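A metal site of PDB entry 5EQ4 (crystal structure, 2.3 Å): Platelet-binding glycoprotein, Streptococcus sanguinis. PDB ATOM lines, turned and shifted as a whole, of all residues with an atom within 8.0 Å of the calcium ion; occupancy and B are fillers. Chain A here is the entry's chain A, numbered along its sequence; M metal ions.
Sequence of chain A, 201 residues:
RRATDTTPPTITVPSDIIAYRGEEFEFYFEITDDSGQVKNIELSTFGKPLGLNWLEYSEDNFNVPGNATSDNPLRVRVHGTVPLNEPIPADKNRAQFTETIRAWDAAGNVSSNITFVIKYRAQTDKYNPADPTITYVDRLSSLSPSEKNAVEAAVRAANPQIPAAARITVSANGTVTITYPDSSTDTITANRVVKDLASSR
The calcium ion is bound by OD2 of Asp 105 (2.4 Å), OD1 of Asp 34 (2.4 Å), OD2 of Asp 33 (2.4 Å), OD1 of Asp 5 (2.4 Å), OD1 of Asp 33 (2.4 Å), O of Thr 7 (2.4 Å) and OD2 of Asp 5 (2.4 Å).
Within 4 Å of the calcium ion: Asp 5, Thr 7, Asp 33, Asp 34 and Asp 105.
The nearest printed residue that does not touch the calcium ion is Ser 35 (4.3 Å).
The side-chain carboxylate (OD1) of Asp 105 is in hydrogen-bond range of the backbone NH (N) of Asn 109, 2.8 Å away.
The side-chain carboxylate of Asp 105 is in hydrogen-bond range of the backbone NH of Ala 107, 3.3 Å away.
The backbone NH (N) of Gly 108 sits at hydrogen-bond distance from the side-chain carboxylate (OD1) of Asp 105 (3.1 Å).
OD2 of Asp 33 sits close to OG of Ser 35.
O of Asp 5 is in hydrogen-bond range of ND2 of Asn 109 (2.9 Å).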
ATOM      1  N   THR A   4      -7.058  23.153 -30.561  1.00  0.00           N
ATOM      2  CA  THR A   4      -6.322  24.413 -30.575  1.00  0.00           C
ATOM      3  C   THR A   4      -5.254  24.437 -29.487  1.00  0.00           C
ATOM      4  O   THR A   4      -5.552  24.241 -28.303  1.00  0.00           O
ATOM      5  CB  THR A   4      -7.277  25.583 -30.404  1.00  0.00           C
ATOM      6  N   ASP A   5      -4.006  24.667 -29.882  1.00  0.00           N
ATOM      7  CA  ASP A   5      -2.897  24.712 -28.935  1.00  0.00           C
ATOM      8  C   ASP A   5      -3.001  25.959 -28.072  1.00  0.00           C
ATOM      9  O   ASP A   5      -2.967  27.081 -28.581  1.00  0.00           O
ATOM     10  CB  ASP A   5      -1.567  24.677 -29.680  1.00  0.00           C
ATOM     11  CG  ASP A   5      -0.379  24.401 -28.775  1.00  0.00           C
ATOM     12  OD1 ASP A   5       0.641  23.878 -29.277  1.00  0.00           O
ATOM     13  OD2 ASP A   5      -0.441  24.691 -27.552  1.00  0.00           O
ATOM     14  N   THR A   6      -3.131  25.755 -26.752  1.00  0.00           N
ATOM     15  CA  THR A   6      -3.071  26.846 -25.796  1.00  0.00           C
ATOM     16  C   THR A   6      -2.046  26.585 -24.693  1.00  0.00           C
ATOM     17  O   THR A   6      -2.008  27.335 -23.711  1.00  0.00           O
ATOM     18  CB  THR A   6      -4.446  27.098 -25.154  1.00  0.00           C
ATOM     19  OG1 THR A   6      -4.863  25.941 -24.425  1.00  0.00           O
ATOM     20  CG2 THR A   6      -5.483  27.414 -26.226  1.00  0.00           C
ATOM     21  N   THR A   7      -1.225  25.538 -24.832  1.00  0.00           N
ATOM     22  CA  THR A   7      -0.256  25.158 -23.813  1.00  0.00           C
ATOM     23  C   THR A   7       1.103  25.735 -24.141  1.00  0.00           C
ATOM     24  O   THR A   7       1.621  25.509 -25.243  1.00  0.00           O
ATOM     25  CB  THR A   7      -0.155  23.634 -23.704  1.00  0.00           C
ATOM     26  OG1 THR A   7      -1.434  23.081 -23.394  1.00  0.00           O
ATOM     27  CG2 THR A   7       0.834  23.245 -22.621  1.00  0.00           C
ATOM     28  N   PRO A   8       1.712  26.490 -23.223  1.00  0.00           N
ATOM     29  CA  PRO A   8       3.040  27.042 -23.475  1.00  0.00           C
ATOM     30  C   PRO A   8       4.100  25.943 -23.408  1.00  0.00           C
ATOM     31  O   PRO A   8       3.863  24.883 -22.828  1.00  0.00           O
ATOM     32  CB  PRO A   8       3.219  28.050 -22.331  1.00  0.00           C
ATOM     33  CG  PRO A   8       2.361  27.517 -21.238  1.00  0.00           C
ATOM     34  CD  PRO A   8       1.176  26.883 -21.908  1.00  0.00           C
ATOM     35  N   PRO A   9       5.271  26.172 -23.995  1.00  0.00           N
ATOM     36  CA  PRO A   9       6.328  25.165 -23.931  1.00  0.00           C
ATOM     37  C   PRO A   9       6.877  25.004 -22.517  1.00  0.00           C
ATOM     38  O   PRO A   9       6.674  25.844 -21.639  1.00  0.00           O
ATOM     39  CB  PRO A   9       7.404  25.719 -24.872  1.00  0.00           C
ATOM     40  CG  PRO A   9       6.687  26.695 -25.762  1.00  0.00           C
ATOM     41  CD  PRO A   9       5.620  27.284 -24.890  1.00  0.00           C
ATOM     42  N   THR A  10       7.576  23.896 -22.319  1.00  0.00           N
ATOM     43  CA  THR A  10       8.201  23.558 -21.040  1.00  0.00           C
ATOM     44  C   THR A  10       9.711  23.636 -21.191  1.00  0.00           C
ATOM     45  O   THR A  10      10.266  23.129 -22.171  1.00  0.00           O
ATOM     46  CB  THR A  10       7.774  22.166 -20.583  1.00  0.00           C
ATOM     47  OG1 THR A  10       6.370  22.164 -20.307  1.00  0.00           O
ATOM     48  CG2 THR A  10       8.521  21.762 -19.320  1.00  0.00           C
ATOM     49  N   THR A  32      10.483  21.662 -24.522  1.00  0.00           N
ATOM     50  CA  THR A  32       9.484  20.774 -25.103  1.00  0.00           C
ATOM     51  C   THR A  32       8.154  21.514 -25.217  1.00  0.00           C
ATOM     52  O   THR A  32       7.861  22.412 -24.436  1.00  0.00           O
ATOM     53  CB  THR A  32       9.260  19.505 -24.263  1.00  0.00           C
ATOM     54  OG1 THR A  32       8.924  19.875 -22.919  1.00  0.00           O
ATOM     55  CG2 THR A  32      10.504  18.647 -24.247  1.00  0.00           C
ATOM     56  N   ASP A  33       7.356  21.104 -26.199  1.00  0.00           N
ATOM     57  CA  ASP A  33       5.994  21.603 -26.353  1.00  0.00           C
ATOM     58  C   ASP A  33       5.090  20.441 -26.747  1.00  0.00           C
ATOM     59  O   ASP A  33       5.534  19.484 -27.388  1.00  0.00           O
ATOM     60  CB  ASP A  33       5.904  22.724 -27.393  1.00  0.00           C
ATOM     61  CG  ASP A  33       4.536  23.388 -27.427  1.00  0.00           C
ATOM     62  OD1 ASP A  33       4.243  24.203 -26.529  1.00  0.00           O
ATOM     63  OD2 ASP A  33       3.754  23.096 -28.354  1.00  0.00           O
ATOM     64  N   ASP A  34       3.822  20.543 -26.345  1.00  0.00           N
ATOM     65  CA  ASP A  34       2.874  19.467 -26.629  1.00  0.00           C
ATOM     66  C   ASP A  34       2.656  19.288 -28.126  1.00  0.00           C
ATOM     67  O   ASP A  34       2.362  18.174 -28.583  1.00  0.00           O
ATOM     68  CB  ASP A  34       1.548  19.753 -25.936  1.00  0.00           C
ATOM     69  CG  ASP A  34       0.974  21.119 -26.283  1.00  0.00           C
ATOM     70  OD1 ASP A  34       1.764  22.009 -26.674  1.00  0.00           O
ATOM     71  OD2 ASP A  34      -0.253  21.299 -26.167  1.00  0.00           O
ATOM     72  N   SER A  35       2.805  20.361 -28.911  1.00  0.00           N
ATOM     73  CA  SER A  35       2.684  20.267 -30.361  1.00  0.00           C
ATOM     74  C   SER A  35       3.909  19.637 -31.014  1.00  0.00           C
ATOM     75  O   SER A  35       3.833  19.255 -32.186  1.00  0.00           O
ATOM     76  CB  SER A  35       2.452  21.654 -30.959  1.00  0.00           C
ATOM     77  OG  SER A  35       3.630  22.448 -30.883  1.00  0.00           O
ATOM     78  N   GLY A  36       5.015  19.514 -30.280  1.00  0.00           N
ATOM     79  CA  GLY A  36       6.246  19.009 -30.857  1.00  0.00           C
ATOM     80  C   GLY A  36       7.066  20.049 -31.601  1.00  0.00           C
ATOM     81  O   GLY A  36       8.044  19.674 -32.253  1.00  0.00           O
ATOM     82  N   GLN A  37       6.700  21.317 -31.526  1.00  0.00           N
ATOM     83  CA  GLN A  37       7.389  22.368 -32.258  1.00  0.00           C
ATOM     84  C   GLN A  37       7.566  23.586 -31.373  1.00  0.00           C
ATOM     85  O   GLN A  37       6.626  24.011 -30.683  1.00  0.00           O
ATOM     86  CB  GLN A  37       6.603  22.750 -33.530  1.00  0.00           C
ATOM     87  CG  GLN A  37       7.231  23.873 -34.329  1.00  0.00           C
ATOM     88  CD  GLN A  37       6.571  24.057 -35.686  1.00  0.00           C
ATOM     89  OE1 GLN A  37       5.860  23.173 -36.165  1.00  0.00           O
ATOM     90  NE2 GLN A  37       6.796  25.217 -36.304  1.00  0.00           N
ATOM     91  N   VAL A  38       8.781  24.138 -31.371  1.00  0.00           N
ATOM     92  CA  VAL A  38       9.099  25.367 -30.640  1.00  0.00           C
ATOM     93  C   VAL A  38       9.623  26.383 -31.644  1.00  0.00           C
ATOM     94  O   VAL A  38      10.520  26.082 -32.434  1.00  0.00           O
ATOM     95  CB  VAL A  38      10.124  25.105 -29.523  1.00  0.00           C
ATOM     96  CG1 VAL A  38      10.753  26.412 -29.054  1.00  0.00           C
ATOM     97  CG2 VAL A  38       9.461  24.397 -28.358  1.00  0.00           C
ATOM     98  N   TRP A 104       8.276  30.166 -27.005  1.00  0.00           N
ATOM     99  CA  TRP A 104       6.912  30.100 -27.510  1.00  0.00           C
ATOM    100  C   TRP A 104       6.852  29.139 -28.694  1.00  0.00           C
ATOM    101  O   TRP A 104       7.857  28.894 -29.382  1.00  0.00           O
ATOM    102  CB  TRP A 104       6.388  31.485 -27.913  1.00  0.00           C
ATOM    103  CG  TRP A 104       7.307  32.272 -28.789  1.00  0.00           C
ATOM    104  CD1 TRP A 104       7.424  32.201 -30.143  1.00  0.00           C
ATOM    105  CD2 TRP A 104       8.225  33.284 -28.366  1.00  0.00           C
ATOM    106  NE1 TRP A 104       8.365  33.091 -30.596  1.00  0.00           N
ATOM    107  CE2 TRP A 104       8.874  33.772 -29.519  1.00  0.00           C
ATOM    108  CE3 TRP A 104       8.576  33.833 -27.120  1.00  0.00           C
ATOM    109  CZ2 TRP A 104       9.847  34.774 -29.464  1.00  0.00           C
ATOM    110  CZ3 TRP A 104       9.538  34.821 -27.066  1.00  0.00           C
ATOM    111  CH2 TRP A 104      10.159  35.280 -28.235  1.00  0.00           C
ATOM    112  N   ASP A 105       5.659  28.592 -28.915  1.00  0.00           N
ATOM    113  CA  ASP A 105       5.427  27.642 -29.993  1.00  0.00           C
ATOM    114  C   ASP A 105       4.951  28.386 -31.246  1.00  0.00           C
ATOM    115  O   ASP A 105       4.968  29.614 -31.310  1.00  0.00           O
ATOM    116  CB  ASP A 105       4.431  26.574 -29.542  1.00  0.00           C
ATOM    117  CG  ASP A 105       3.178  27.162 -28.905  1.00  0.00           C
ATOM    118  OD1 ASP A 105       2.848  28.327 -29.195  1.00  0.00           O
ATOM    119  OD2 ASP A 105       2.528  26.442 -28.109  1.00  0.00           O
ATOM    120  N   ALA A 106       4.503  27.633 -32.254  1.00  0.00           N
ATOM    121  CA  ALA A 106       3.999  28.261 -33.469  1.00  0.00           C
ATOM    122  C   ALA A 106       2.629  28.878 -33.257  1.00  0.00           C
ATOM    123  O   ALA A 106       2.260  29.827 -33.961  1.00  0.00           O
ATOM    124  CB  ALA A 106       3.950  27.234 -34.606  1.00  0.00           C
ATOM    125  N   ALA A 107       1.852  28.374 -32.296  1.00  0.00           N
ATOM    126  CA  ALA A 107       0.523  28.906 -32.045  1.00  0.00           C
ATOM    127  C   ALA A 107       0.558  30.272 -31.367  1.00  0.00           C
ATOM    128  O   ALA A 107      -0.462  30.965 -31.360  1.00  0.00           O
ATOM    129  CB  ALA A 107      -0.289  27.918 -31.199  1.00  0.00           C
ATOM    130  N   GLY A 108       1.692  30.661 -30.800  1.00  0.00           N
ATOM    131  CA  GLY A 108       1.809  31.922 -30.119  1.00  0.00           C
ATOM    132  C   GLY A 108       1.644  31.871 -28.615  1.00  0.00           C
ATOM    133  O   GLY A 108       1.249  32.881 -28.022  1.00  0.00           O
ATOM    134  N   ASN A 109       1.938  30.732 -27.984  1.00  0.00           N
ATOM    135  CA  ASN A 109       1.846  30.580 -26.534  1.00  0.00           C
ATOM    136  C   ASN A 109       3.249  30.636 -25.965  1.00  0.00           C
ATOM    137  O   ASN A 109       4.066  29.742 -26.203  1.00  0.00           O
ATOM    138  CB  ASN A 109       1.148  29.269 -26.175  1.00  0.00           C
ATOM    139  CG  ASN A 109      -0.212  29.126 -26.826  1.00  0.00           C
ATOM    140  OD1 ASN A 109      -1.048  30.025 -26.730  1.00  0.00           O
ATOM    141  ND2 ASN A 109      -0.433  28.003 -27.501  1.00  0.00           N
ATOM    142  N   VAL A 110       3.541  31.686 -25.193  1.00  0.00           N
ATOM    143  CA  VAL A 110       4.859  31.895 -24.618  1.00  0.00           C
ATOM    144  C   VAL A 110       4.878  31.364 -23.184  1.00  0.00           C
ATOM    145  O   VAL A 110       3.924  31.565 -22.427  1.00  0.00           O
ATOM    146  CB  VAL A 110       5.259  33.389 -24.667  1.00  0.00           C
ATOM    147  CG1 VAL A 110       4.217  34.249 -23.973  1.00  0.00           C
ATOM    148  CG2 VAL A 110       6.637  33.598 -24.049  1.00  0.00           C
HETATM  149 CA    CA M   1       1.958  24.294 -27.305  1.00  0.00          CA
